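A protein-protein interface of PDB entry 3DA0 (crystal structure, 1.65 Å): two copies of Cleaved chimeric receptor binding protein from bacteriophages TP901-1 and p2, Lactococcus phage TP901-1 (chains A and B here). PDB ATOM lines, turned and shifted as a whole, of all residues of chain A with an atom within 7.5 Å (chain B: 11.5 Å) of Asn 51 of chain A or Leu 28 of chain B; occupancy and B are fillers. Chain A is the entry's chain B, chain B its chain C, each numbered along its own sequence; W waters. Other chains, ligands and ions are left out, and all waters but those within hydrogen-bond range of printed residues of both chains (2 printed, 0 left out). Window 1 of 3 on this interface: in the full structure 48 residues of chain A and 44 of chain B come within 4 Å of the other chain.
N of Thr 29 of chain A lies within hydrogen-bond range of O of Val 22 of chain B, 2.8 Å away. The backbone NH (N) of Val 24 of chain B sits at hydrogen-bond distance from the backbone carbonyl oxygen (O) of Thr 29 of chain A, at 2.9 Å. The side-chain amide nitrogen (ND2) of Asn 51 of chain A sits at hydrogen-bond distance from the backbone carbonyl oxygen (O) of Leu 28 of chain B, at 2.8 Å. NZ of Lys 50 of chain B lies within salt-bridge range of OD2 of Asp 53 of chain A, at 2.5 Å. The backbone carbonyl oxygen (O) of Lys 133 of chain A sits at hydrogen-bond distance from the side-chain amino group (NZ) of Lys 50 of chain B (2.7 Å).
The backbone carbonyl oxygen of Pro 31 of chain A sits at hydrogen-bond distance from the backbone NH of Asn 51 of chain A (2.8 Å). The backbone NH of Ile 132 of chain A is in hydrogen-bond range of the backbone carbonyl oxygen of Asp 53 of chain A (2.8 Å). The backbone NH (N) of Lys 133 of chain A lies within hydrogen-bond range of the side-chain carboxylate (OD1) of Asp 53 of chain A, 3.0 Å away. OD1 of Asn 25 of chain B sits close to OE2 of Glu 23 of chain B, 2.9 Å away.
Among the printed residues, merely in contact across the chains: Phe 18 of chain A with Ile 12 of chain B (3.3 Å), Phe 18 of chain A with Lys 16 of chain B (3.8 Å), Val 22 of chain A with Lys 16 of chain B (3.4 Å), Val 22 of chain A with Phe 18 of chain B (3.8 Å), Leu 28 of chain A with Val 22 of chain B (3.3 Å), Thr 29 of chain A with Glu 23 of chain B (3.3 Å), Leu 30 of chain A with Val 24 of chain B (3.8 Å), Leu 30 of chain A with Leu 28 of chain B (3.9 Å), Pro 31 of chain A with Val 24 of chain B (3.3 Å), Pro 31 of chain A with Asn 25 of chain B (3.7 Å), Pro 31 of chain A with Gly 26 of chain B (3.2 Å) and Asn 51 of chain A with Ser 27 of chain B (3.7 Å).
Of the printed residues of chain A, Leu 28 of chain B touches Leu 30 (3.9 Å) and Asn 51 (2.8 Å). Of chain B, only Val 24, Asn 25 and Gly 26 come within 4 Å of Pro 31 of chain A. No residue of chain B comes within 4 Å of Val 32 of chain A. No residue of chain B comes within 4 Å of Lys 49 of chain A. No residue of chain B comes within 4 Å of Asn 52 of chain A. Of chain B, only Lys 50 (2.5 Å) comes within 4 Å of Asp 53 of chain A. Printed residues of chain A within 4 Å of Phe 18 of chain B: Val 22. Of the printed residues of chain A, Ser 27 of chain B touches Asn 51. Lys 49 of chain B touches none of the printed residues of chain A. Lys 50 of chain A touches none of the printed residues of chain B. The nearest residue of chain B that does not touch Asn 51 of chain A is Gly 26 of chain B (4.2 Å). The nearest printed residue of chain A that does not touch Leu 28 of chain B is Leu 28 of chain A (4.01 Å). The nearest printed residue of chain B that does not touch Val 22 of chain A is Val 22 of chain B (6.6 Å).
Among the printed residues, 17 pairs touch across the chains.
Phe 18 of chain A touches Lys 16 of chain B, but with the chains exchanged Lys 16 of chain A does not touch Phe 18 of chain B (8.2 Å). Val 22 of chain A touches Phe 18 of chain B, but with the chains exchanged Phe 18 of chain A does not touch Val 22 of chain B (7.6 Å). Leu 28 of chain A touches Val 22 of chain B, but with the chains exchanged Val 22 of chain A does not touch Leu 28 of chain B (7.3 Å). Asn 51 of chain A touches Leu 28 of chain B, but with the chains exchanged Leu 28 of chain A does not touch Asn 51 of chain B (8.2 Å). Positions printed for both chains: 16, 18, 22, 28, 29, 30, 31, 32, 49, 50, 51, 52 and 54.
Water W2 lies within hydrogen-bond range of the side-chain hydroxyl of Thr 29 of chain A and the backbone carbonyl oxygen of Val 22 of chain B. Water W1 bridges the backbone carbonyl oxygen (O) of Asn 25 of chain B (2.8 Å) and the side-chain amide oxygen (OD1) of Asn 52 of chain A (3.1 Å).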
ATOM      1  N   LYS A  16      -4.818 -13.519  28.097  1.00  0.00           N
ATOM      2  CA  LYS A  16      -5.401 -13.930  26.850  1.00  0.00           C
ATOM      3  C   LYS A  16      -5.102 -12.851  25.833  1.00  0.00           C
ATOM      4  O   LYS A  16      -5.498 -11.718  25.987  1.00  0.00           O
ATOM      5  CB  LYS A  16      -6.904 -14.149  26.975  1.00  0.00           C
ATOM      6  CG  LYS A  16      -7.267 -15.156  28.048  1.00  0.00           C
ATOM      7  CD  LYS A  16      -6.673 -16.513  27.915  1.00  0.00           C
ATOM      8  CE  LYS A  16      -7.401 -17.479  28.851  1.00  0.00           C
ATOM      9  NZ  LYS A  16      -6.605 -18.740  28.956  1.00  0.00           N
ATOM     10  N   PHE A  18      -5.750 -11.732  22.033  1.00  0.00           N
ATOM     11  CA  PHE A  18      -6.541 -11.884  20.814  1.00  0.00           C
ATOM     12  C   PHE A  18      -5.757 -11.195  19.721  1.00  0.00           C
ATOM     13  O   PHE A  18      -5.590 -10.000  19.746  1.00  0.00           O
ATOM     14  CB  PHE A  18      -7.923 -11.277  20.973  1.00  0.00           C
ATOM     15  CG  PHE A  18      -8.751 -11.985  21.999  1.00  0.00           C
ATOM     16  CD1 PHE A  18      -8.638 -11.631  23.319  1.00  0.00           C
ATOM     17  CD2 PHE A  18      -9.672 -12.956  21.632  1.00  0.00           C
ATOM     18  CE1 PHE A  18      -9.414 -12.263  24.301  1.00  0.00           C
ATOM     19  CE2 PHE A  18     -10.447 -13.627  22.600  1.00  0.00           C
ATOM     20  CZ  PHE A  18     -10.321 -13.256  23.934  1.00  0.00           C
ATOM     21  N   VAL A  22     -11.804  -8.156  17.897  1.00  0.00           N
ATOM     22  CA  VAL A  22     -12.736  -8.558  18.947  1.00  0.00           C
ATOM     23  C   VAL A  22     -13.895  -7.590  18.901  1.00  0.00           C
ATOM     24  O   VAL A  22     -13.709  -6.394  18.711  1.00  0.00           O
ATOM     25  CB  VAL A  22     -12.080  -8.575  20.346  1.00  0.00           C
ATOM     26  CG1 VAL A  22     -13.124  -8.888  21.451  1.00  0.00           C
ATOM     27  CG2 VAL A  22     -10.948  -9.621  20.400  1.00  0.00           C
ATOM     28  N   LEU A  28     -18.920  -3.816  27.952  1.00  0.00           N
ATOM     29  CA  LEU A  28     -17.582  -4.185  28.348  1.00  0.00           C
ATOM     30  C   LEU A  28     -17.309  -3.435  29.648  1.00  0.00           C
ATOM     31  O   LEU A  28     -17.386  -2.212  29.669  1.00  0.00           O
ATOM     32  CB  LEU A  28     -16.607  -3.780  27.271  1.00  0.00           C
ATOM     33  CG  LEU A  28     -15.132  -3.900  27.638  1.00  0.00           C
ATOM     34  CD1 LEU A  28     -14.808  -5.331  27.920  1.00  0.00           C
ATOM     35  CD2 LEU A  28     -14.229  -3.400  26.490  1.00  0.00           C
ATOM     36  N   THR A  29     -17.067  -4.170  30.739  1.00  0.00           N
ATOM     37  CA  THR A  29     -16.775  -3.603  32.058  1.00  0.00           C
ATOM     38  C   THR A  29     -15.268  -3.711  32.272  1.00  0.00           C
ATOM     39  O   THR A  29     -14.685  -4.772  32.206  1.00  0.00           O
ATOM     40  CB  THR A  29     -17.510  -4.356  33.166  1.00  0.00           C
ATOM     41  OG1 THR A  29     -18.924  -4.266  32.935  1.00  0.00           O
ATOM     42  CG2 THR A  29     -17.166  -3.812  34.571  1.00  0.00           C
ATOM     43  N   LEU A  30     -14.643  -2.561  32.502  1.00  0.00           N
ATOM     44  CA  LEU A  30     -13.224  -2.456  32.792  1.00  0.00           C
ATOM     45  C   LEU A  30     -13.085  -1.899  34.208  1.00  0.00           C
ATOM     46  O   LEU A  30     -14.078  -1.406  34.787  1.00  0.00           O
ATOM     47  CB  LEU A  30     -12.470  -1.537  31.789  1.00  0.00           C
ATOM     48  CG  LEU A  30     -12.622  -1.963  30.305  1.00  0.00           C
ATOM     49  CD1 LEU A  30     -12.040  -0.949  29.324  1.00  0.00           C
ATOM     50  CD2 LEU A  30     -12.012  -3.306  30.027  1.00  0.00           C
ATOM     51  N   PRO A  31     -11.880  -2.018  34.779  1.00  0.00           N
ATOM     52  CA  PRO A  31     -11.622  -1.450  36.107  1.00  0.00           C
ATOM     53  C   PRO A  31     -11.939   0.025  36.129  1.00  0.00           C
ATOM     54  O   PRO A  31     -11.617   0.719  35.191  1.00  0.00           O
ATOM     55  CB  PRO A  31     -10.124  -1.665  36.309  1.00  0.00           C
ATOM     56  CG  PRO A  31      -9.775  -2.791  35.356  1.00  0.00           C
ATOM     57  CD  PRO A  31     -10.669  -2.664  34.213  1.00  0.00           C
ATOM     58  N   VAL A  32     -12.507   0.474  37.241  1.00  0.00           N
ATOM     59  CA  VAL A  32     -12.811   1.881  37.403  1.00  0.00           C
ATOM     60  C   VAL A  32     -12.386   2.255  38.817  1.00  0.00           C
ATOM     61  O   VAL A  32     -12.679   1.500  39.750  1.00  0.00           O
ATOM     62  CB  VAL A  32     -14.277   2.156  37.256  1.00  0.00           C
ATOM     63  CG1 VAL A  32     -14.577   3.640  37.493  1.00  0.00           C
ATOM     64  CG2 VAL A  32     -14.736   1.777  35.862  1.00  0.00           C
ATOM     65  N   GLN A  33     -11.697   3.384  38.979  1.00  0.00           N
ATOM     66  CA  GLN A  33     -11.355   3.900  40.295  1.00  0.00           C
ATOM     67  C   GLN A  33     -11.664   5.376  40.262  1.00  0.00           C
ATOM     68  O   GLN A  33     -11.475   6.009  39.232  1.00  0.00           O
ATOM     69  CB  GLN A  33      -9.873   3.659  40.563  1.00  0.00           C
ATOM     70  CG  GLN A  33      -9.445   3.701  42.016  1.00  0.00           C
ATOM     71  CD  GLN A  33      -7.948   3.374  42.231  1.00  0.00           C
ATOM     72  OE1 GLN A  33      -7.168   3.191  41.290  1.00  0.00           O
ATOM     73  NE2 GLN A  33      -7.549   3.316  43.490  1.00  0.00           N
ATOM     74  N   LYS A  49     -10.911   7.087  36.673  1.00  0.00           N
ATOM     75  CA  LYS A  49      -9.899   6.393  35.914  1.00  0.00           C
ATOM     76  C   LYS A  49     -10.434   5.066  35.447  1.00  0.00           C
ATOM     77  O   LYS A  49     -10.915   4.284  36.273  1.00  0.00           O
ATOM     78  CB  LYS A  49      -8.691   6.139  36.825  1.00  0.00           C
ATOM     79  CG  LYS A  49      -7.599   5.338  36.174  1.00  0.00           C
ATOM     80  CD  LYS A  49      -6.362   5.253  37.047  1.00  0.00           C
ATOM     81  CE  LYS A  49      -6.686   4.730  38.417  1.00  0.00           C
ATOM     82  NZ  LYS A  49      -6.750   3.303  38.421  1.00  0.00           N
ATOM     83  N   LYS A  50     -10.411   4.841  34.146  1.00  0.00           N
ATOM     84  CA  LYS A  50     -10.879   3.572  33.611  1.00  0.00           C
ATOM     85  C   LYS A  50      -9.741   2.783  32.995  1.00  0.00           C
ATOM     86  O   LYS A  50      -8.826   3.308  32.318  1.00  0.00           O
ATOM     87  CB  LYS A  50     -12.000   3.831  32.608  1.00  0.00           C
ATOM     88  CG  LYS A  50     -13.195   4.477  33.335  1.00  0.00           C
ATOM     89  CD  LYS A  50     -14.565   4.014  32.961  1.00  0.00           C
ATOM     90  CE  LYS A  50     -15.552   4.915  33.627  1.00  0.00           C
ATOM     91  NZ  LYS A  50     -17.028   4.569  33.405  1.00  0.00           N
ATOM     92  N   ASN A  51      -9.780   1.492  33.257  1.00  0.00           N
ATOM     93  CA  ASN A  51      -8.772   0.568  32.726  1.00  0.00           C
ATOM     94  C   ASN A  51      -7.339   0.926  33.126  1.00  0.00           C
ATOM     95  O   ASN A  51      -6.366   0.708  32.365  1.00  0.00           O
ATOM     96  CB  ASN A  51      -8.915   0.506  31.197  1.00  0.00           C
ATOM     97  CG  ASN A  51      -8.158  -0.662  30.601  1.00  0.00           C
ATOM     98  OD1 ASN A  51      -8.117  -1.722  31.180  1.00  0.00           O
ATOM     99  ND2 ASN A  51      -7.494  -0.443  29.465  1.00  0.00           N
ATOM    100  N   ASN A  52      -7.181   1.510  34.316  1.00  0.00           N
ATOM    101  CA  ASN A  52      -5.882   1.999  34.807  1.00  0.00           C
ATOM    102  C   ASN A  52      -5.164   2.875  33.819  1.00  0.00           C
ATOM    103  O   ASN A  52      -3.946   2.966  33.811  1.00  0.00           O
ATOM    104  CB  ASN A  52      -4.990   0.795  35.226  1.00  0.00           C
ATOM    105  CG  ASN A  52      -5.636  -0.060  36.289  1.00  0.00           C
ATOM    106  OD1 ASN A  52      -5.832  -1.294  36.104  1.00  0.00           O
ATOM    107  ND2 ASN A  52      -5.998   0.555  37.384  1.00  0.00           N
ATOM    108  N   ASP A  53      -5.953   3.640  33.043  1.00  0.00           N
ATOM    109  CA  ASP A  53      -5.394   4.343  31.899  1.00  0.00           C
ATOM    110  C   ASP A  53      -6.077   5.649  31.562  1.00  0.00           C
ATOM    111  O   ASP A  53      -5.496   6.704  31.755  1.00  0.00           O
ATOM    112  CB  ASP A  53      -5.399   3.455  30.704  1.00  0.00           C
ATOM    113  CG  ASP A  53      -4.728   4.110  29.502  1.00  0.00           C
ATOM    114  OD1 ASP A  53      -3.902   5.026  29.666  1.00  0.00           O
ATOM    115  OD2 ASP A  53      -5.041   3.718  28.391  1.00  0.00           O
ATOM    116  N   LEU A  54      -7.317   5.600  31.081  1.00  0.00           N
ATOM    117  CA  LEU A  54      -8.006   6.829  30.700  1.00  0.00           C
ATOM    118  C   LEU A  54      -8.555   7.515  31.971  1.00  0.00           C
ATOM    119  O   LEU A  54      -9.352   6.929  32.700  1.00  0.00           O
ATOM    120  CB  LEU A  54      -9.175   6.451  29.760  1.00  0.00           C
ATOM    121  CG  LEU A  54      -9.991   7.648  29.297  1.00  0.00           C
ATOM    122  CD1 LEU A  54      -9.188   8.728  28.530  1.00  0.00           C
ATOM    123  CD2 LEU A  54     -11.220   7.112  28.507  1.00  0.00           C
ATOM    124  N   ILE A 132      -2.903   7.773  31.328  1.00  0.00           N
ATOM    125  CA  ILE A 132      -1.776   7.443  32.205  1.00  0.00           C
ATOM    126  C   ILE A 132      -0.731   6.792  31.343  1.00  0.00           C
ATOM    127  O   ILE A 132       0.441   7.069  31.523  1.00  0.00           O
ATOM    128  CB  ILE A 132      -2.232   6.605  33.382  1.00  0.00           C
ATOM    129  CG1 ILE A 132      -3.075   7.511  34.314  1.00  0.00           C
ATOM    130  CG2 ILE A 132      -1.028   5.927  34.071  1.00  0.00           C
ATOM    131  CD1 ILE A 132      -3.846   6.694  35.363  1.00  0.00           C
ATOM    132  N   LYS A 133      -1.168   5.895  30.442  1.00  0.00           N
ATOM    133  CA  LYS A 133      -0.273   5.207  29.497  1.00  0.00           C
ATOM    134  C   LYS A 133      -0.354   5.943  28.167  1.00  0.00           C
ATOM    135  O   LYS A 133      -0.979   5.492  27.234  1.00  0.00           O
ATOM    136  CB  LYS A 133      -0.697   3.773  29.385  1.00  0.00           C
ATOM    137  CG  LYS A 133      -0.585   3.048  30.725  1.00  0.00           C
ATOM    138  CD  LYS A 133      -0.893   1.588  30.597  1.00  0.00           C
ATOM    139  CE  LYS A 133      -1.323   0.959  31.906  1.00  0.00           C
ATOM    140  NZ  LYS A 133      -1.688  -0.489  31.759  1.00  0.00           N
ATOM    141  N   ILE B  12      -4.893 -16.169  20.829  1.00  0.00           N
ATOM    142  CA  ILE B  12      -6.197 -16.551  20.268  1.00  0.00           C
ATOM    143  C   ILE B  12      -6.422 -15.789  18.964  1.00  0.00           C
ATOM    144  O   ILE B  12      -6.513 -14.566  18.976  1.00  0.00           O
ATOM    145  CB  ILE B  12      -7.360 -16.191  21.237  1.00  0.00           C
ATOM    146  CG1 ILE B  12      -7.153 -16.878  22.580  1.00  0.00           C
ATOM    147  CG2 ILE B  12      -8.709 -16.544  20.625  1.00  0.00           C
ATOM    148  CD1 ILE B  12      -8.005 -16.302  23.677  1.00  0.00           C
ATOM    149  N   LYS B  16     -13.434 -12.737  17.400  1.00  0.00           N
ATOM    150  CA  LYS B  16     -14.273 -13.231  18.451  1.00  0.00           C
ATOM    151  C   LYS B  16     -15.297 -12.146  18.759  1.00  0.00           C
ATOM    152  O   LYS B  16     -14.977 -11.062  19.204  1.00  0.00           O
ATOM    153  CB  LYS B  16     -13.432 -13.604  19.677  1.00  0.00           C
ATOM    154  CG  LYS B  16     -12.338 -14.603  19.429  1.00  0.00           C
ATOM    155  CD  LYS B  16     -12.786 -15.908  18.719  1.00  0.00           C
ATOM    156  CE  LYS B  16     -11.596 -16.849  18.625  1.00  0.00           C
ATOM    157  NZ  LYS B  16     -11.805 -18.090  17.786  1.00  0.00           N
ATOM    158  N   PHE B  18     -18.251 -11.266  21.110  1.00  0.00           N
ATOM    159  CA  PHE B  18     -18.881 -11.562  22.376  1.00  0.00           C
ATOM    160  C   PHE B  18     -20.229 -10.868  22.327  1.00  0.00           C
ATOM    161  O   PHE B  18     -20.316  -9.648  22.367  1.00  0.00           O
ATOM    162  CB  PHE B  18     -18.035 -11.039  23.529  1.00  0.00           C
ATOM    163  CG  PHE B  18     -16.761 -11.773  23.688  1.00  0.00           C
ATOM    164  CD1 PHE B  18     -15.631 -11.366  22.976  1.00  0.00           C
ATOM    165  CD2 PHE B  18     -16.680 -12.873  24.520  1.00  0.00           C
ATOM    166  CE1 PHE B  18     -14.471 -12.050  23.115  1.00  0.00           C
ATOM    167  CE2 PHE B  18     -15.502 -13.577  24.667  1.00  0.00           C
ATOM    168  CZ  PHE B  18     -14.419 -13.208  23.954  1.00  0.00           C
ATOM    169  N   VAL B  22     -18.889  -8.520  28.715  1.00  0.00           N
ATOM    170  CA  VAL B  22     -17.542  -8.936  28.983  1.00  0.00           C
ATOM    171  C   VAL B  22     -17.020  -8.073  30.124  1.00  0.00           C
ATOM    172  O   VAL B  22     -17.312  -6.896  30.169  1.00  0.00           O
ATOM    173  CB  VAL B  22     -16.680  -8.836  27.728  1.00  0.00           C
ATOM    174  CG1 VAL B  22     -15.230  -9.091  28.061  1.00  0.00           C
ATOM    175  CG2 VAL B  22     -17.191  -9.822  26.613  1.00  0.00           C
ATOM    176  N   GLU B  23     -16.324  -8.681  31.073  1.00  0.00           N
ATOM    177  CA  GLU B  23     -15.694  -7.937  32.172  1.00  0.00           C
ATOM    178  C   GLU B  23     -14.229  -8.304  32.140  1.00  0.00           C
ATOM    179  O   GLU B  23     -13.890  -9.464  31.943  1.00  0.00           O
ATOM    180  CB  GLU B  23     -16.331  -8.303  33.507  1.00  0.00           C
ATOM    181  CG  GLU B  23     -15.621  -7.714  34.745  1.00  0.00           C
ATOM    182  CD  GLU B  23     -16.411  -7.923  36.026  1.00  0.00           C
ATOM    183  OE1 GLU B  23     -17.649  -8.062  35.947  1.00  0.00           O
ATOM    184  OE2 GLU B  23     -15.798  -7.920  37.122  1.00  0.00           O
ATOM    185  N   VAL B  24     -13.364  -7.300  32.247  1.00  0.00           N
ATOM    186  CA  VAL B  24     -11.931  -7.492  32.374  1.00  0.00           C
ATOM    187  C   VAL B  24     -11.544  -6.898  33.729  1.00  0.00           C
ATOM    188  O   VAL B  24     -11.807  -5.732  34.002  1.00  0.00           O
ATOM    189  CB  VAL B  24     -11.158  -6.858  31.225  1.00  0.00           C
ATOM    190  CG1 VAL B  24      -9.629  -7.089  31.379  1.00  0.00           C
ATOM    191  CG2 VAL B  24     -11.645  -7.471  29.893  1.00  0.00           C
ATOM    192  N   ASN B  25     -11.042  -7.753  34.613  1.00  0.00           N
ATOM    193  CA  ASN B  25     -10.516  -7.326  35.917  1.00  0.00           C
ATOM    194  C   ASN B  25      -9.077  -6.874  35.934  1.00  0.00           C
ATOM    195  O   ASN B  25      -8.690  -6.065  36.787  1.00  0.00           O
ATOM    196  CB  ASN B  25     -10.596  -8.473  36.917  1.00  0.00           C
ATOM    197  CG  ASN B  25     -11.961  -8.913  37.155  1.00  0.00           C
ATOM    198  OD1 ASN B  25     -12.902  -8.138  37.045  1.00  0.00           O
ATOM    199  ND2 ASN B  25     -12.103 -10.176  37.548  1.00  0.00           N
ATOM    200  N   GLY B  26      -8.264  -7.410  35.041  1.00  0.00           N
ATOM    201  CA  GLY B  26      -6.918  -6.894  34.842  1.00  0.00           C
ATOM    202  C   GLY B  26      -6.933  -5.687  33.934  1.00  0.00           C
ATOM    203  O   GLY B  26      -7.861  -4.886  33.968  1.00  0.00           O
ATOM    204  N   SER B  27      -5.904  -5.570  33.105  1.00  0.00           N
ATOM    205  CA  SER B  27      -5.774  -4.463  32.190  1.00  0.00           C
ATOM    206  C   SER B  27      -6.229  -4.992  30.823  1.00  0.00           C
ATOM    207  O   SER B  27      -6.006  -6.144  30.518  1.00  0.00           O
ATOM    208  CB  SER B  27      -4.304  -4.107  32.078  1.00  0.00           C
ATOM    209  OG  SER B  27      -3.585  -5.339  31.939  1.00  0.00           O
ATOM    210  N   LEU B  28      -6.887  -4.154  30.039  1.00  0.00           N
ATOM    211  CA  LEU B  28      -7.152  -4.444  28.665  1.00  0.00           C
ATOM    212  C   LEU B  28      -6.171  -3.626  27.871  1.00  0.00           C
ATOM    213  O   LEU B  28      -6.120  -2.434  28.045  1.00  0.00           O
ATOM    214  CB  LEU B  28      -8.549  -3.989  28.300  1.00  0.00           C
ATOM    215  CG  LEU B  28      -8.859  -4.038  26.810  1.00  0.00           C
ATOM    216  CD1 LEU B  28      -8.767  -5.537  26.292  1.00  0.00           C
ATOM    217  CD2 LEU B  28     -10.217  -3.374  26.562  1.00  0.00           C
ATOM    218  N   THR B  29      -5.360  -4.273  27.049  1.00  0.00           N
ATOM    219  CA  THR B  29      -4.394  -3.606  26.234  1.00  0.00           C
ATOM    220  C   THR B  29      -4.891  -3.633  24.813  1.00  0.00           C
ATOM    221  O   THR B  29      -5.150  -4.668  24.265  1.00  0.00           O
ATOM    222  CB  THR B  29      -2.989  -4.299  26.316  1.00  0.00           C
ATOM    223  OG1 THR B  29      -2.525  -4.297  27.668  1.00  0.00           O
ATOM    224  CG2 THR B  29      -1.954  -3.533  25.524  1.00  0.00           C
ATOM    225  N   LEU B  30      -4.977  -2.452  24.218  1.00  0.00           N
ATOM    226  CA  LEU B  30      -5.365  -2.269  22.839  1.00  0.00           C
ATOM    227  C   LEU B  30      -4.208  -1.620  22.067  1.00  0.00           C
ATOM    228  O   LEU B  30      -3.240  -1.184  22.667  1.00  0.00           O
ATOM    229  CB  LEU B  30      -6.582  -1.350  22.774  1.00  0.00           C
ATOM    230  CG  LEU B  30      -7.822  -1.799  23.570  1.00  0.00           C
ATOM    231  CD1 LEU B  30      -8.995  -0.918  23.226  1.00  0.00           C
ATOM    232  CD2 LEU B  30      -8.084  -3.224  23.189  1.00  0.00           C
ATOM    233  N   PRO B  31      -4.291  -1.599  20.726  1.00  0.00           N
ATOM    234  CA  PRO B  31      -3.175  -0.977  19.984  1.00  0.00           C
ATOM    235  C   PRO B  31      -3.036   0.479  20.361  1.00  0.00           C
ATOM    236  O   PRO B  31      -4.025   1.148  20.521  1.00  0.00           O
ATOM    237  CB  PRO B  31      -3.603  -1.155  18.531  1.00  0.00           C
ATOM    238  CG  PRO B  31      -4.400  -2.445  18.584  1.00  0.00           C
ATOM    239  CD  PRO B  31      -5.242  -2.219  19.803  1.00  0.00           C
ATOM    240  N   VAL B  32      -1.790   0.941  20.452  1.00  0.00           N
ATOM    241  CA  VAL B  32      -1.482   2.343  20.753  1.00  0.00           C
ATOM    242  C   VAL B  32      -0.414   2.832  19.773  1.00  0.00           C
ATOM    243  O   VAL B  32       0.535   2.119  19.469  1.00  0.00           O
ATOM    244  CB  VAL B  32      -0.929   2.507  22.183  1.00  0.00           C
ATOM    245  CG1 VAL B  32      -0.529   3.971  22.450  1.00  0.00           C
ATOM    246  CG2 VAL B  32      -1.944   2.000  23.209  1.00  0.00           C
ATOM    247  N   LYS B  49      -3.088   7.662  20.112  1.00  0.00           N
ATOM    248  CA  LYS B  49      -4.246   7.006  19.547  1.00  0.00           C
ATOM    249  C   LYS B  49      -4.336   5.628  20.100  1.00  0.00           C
ATOM    250  O   LYS B  49      -3.358   4.886  20.011  1.00  0.00           O
ATOM    251  CB  LYS B  49      -4.064   6.940  18.024  1.00  0.00           C
ATOM    252  CG  LYS B  49      -5.194   6.257  17.294  1.00  0.00           C
ATOM    253  CD  LYS B  49      -5.013   6.276  15.768  1.00  0.00           C
ATOM    254  CE  LYS B  49      -3.725   5.532  15.394  1.00  0.00           C
ATOM    255  NZ  LYS B  49      -3.839   4.793  14.133  1.00  0.00           N
ATOM    256  N   LYS B  50      -5.515   5.278  20.632  1.00  0.00           N
ATOM    257  CA  LYS B  50      -5.696   3.931  21.137  1.00  0.00           C
ATOM    258  C   LYS B  50      -6.837   3.280  20.408  1.00  0.00           C
ATOM    259  O   LYS B  50      -7.839   3.918  20.065  1.00  0.00           O
ATOM    260  CB  LYS B  50      -5.981   3.992  22.633  1.00  0.00           C
ATOM    261  CG  LYS B  50      -4.812   4.577  23.385  1.00  0.00           C
ATOM    262  CD  LYS B  50      -4.715   4.000  24.781  1.00  0.00           C
ATOM    263  CE  LYS B  50      -3.539   4.645  25.463  1.00  0.00           C
ATOM    264  NZ  LYS B  50      -3.117   3.973  26.748  1.00  0.00           N
ATOM    265  N   ASN B  51      -6.686   1.978  20.132  1.00  0.00           N
ATOM    266  CA  ASN B  51      -7.667   1.214  19.371  1.00  0.00           C
ATOM    267  C   ASN B  51      -7.987   1.825  18.009  1.00  0.00           C
ATOM    268  O   ASN B  51      -9.110   1.687  17.512  1.00  0.00           O
ATOM    269  CB  ASN B  51      -8.945   1.059  20.167  1.00  0.00           C
ATOM    270  CG  ASN B  51      -9.822  -0.095  19.649  1.00  0.00           C
ATOM    271  OD1 ASN B  51      -9.324  -1.099  19.138  1.00  0.00           O
ATOM    272  ND2 ASN B  51     -11.143   0.082  19.766  1.00  0.00           N
ATOM    273  N   ASN B  52      -7.000   2.490  17.413  1.00  0.00           N
ATOM    274  CA  ASN B  52      -7.189   3.142  16.130  1.00  0.00           C
ATOM    275  C   ASN B  52      -8.501   3.930  16.115  1.00  0.00           C
ATOM    276  O   ASN B  52      -9.225   3.988  15.108  1.00  0.00           O
ATOM    277  CB  ASN B  52      -7.158   2.098  15.008  1.00  0.00           C
ATOM    278  CG  ASN B  52      -5.750   1.533  14.790  1.00  0.00           C
ATOM    279  OD1 ASN B  52      -4.851   2.265  14.406  1.00  0.00           O
ATOM    280  ND2 ASN B  52      -5.559   0.257  15.066  1.00  0.00           N
ATOM    281  N   LEU B  54      -9.657   6.322  19.569  1.00  0.00           N
ATOM    282  CA  LEU B  54      -9.649   7.410  20.525  1.00  0.00           C
ATOM    283  C   LEU B  54      -8.276   8.070  20.477  1.00  0.00           C
ATOM    284  O   LEU B  54      -7.270   7.444  20.692  1.00  0.00           O
ATOM    285  CB  LEU B  54      -9.909   6.949  21.962  1.00  0.00           C
ATOM    286  CG  LEU B  54      -9.931   7.989  23.044  1.00  0.00           C
ATOM    287  CD1 LEU B  54     -10.999   9.122  22.835  1.00  0.00           C
ATOM    288  CD2 LEU B  54     -10.143   7.257  24.373  1.00  0.00           C
HETATM  289  O   HOH W   1      -6.857  -3.958  37.246  1.00  0.00           O
HETATM  290  O   HOH W   2     -19.908  -6.107  31.313  1.00  0.00           O
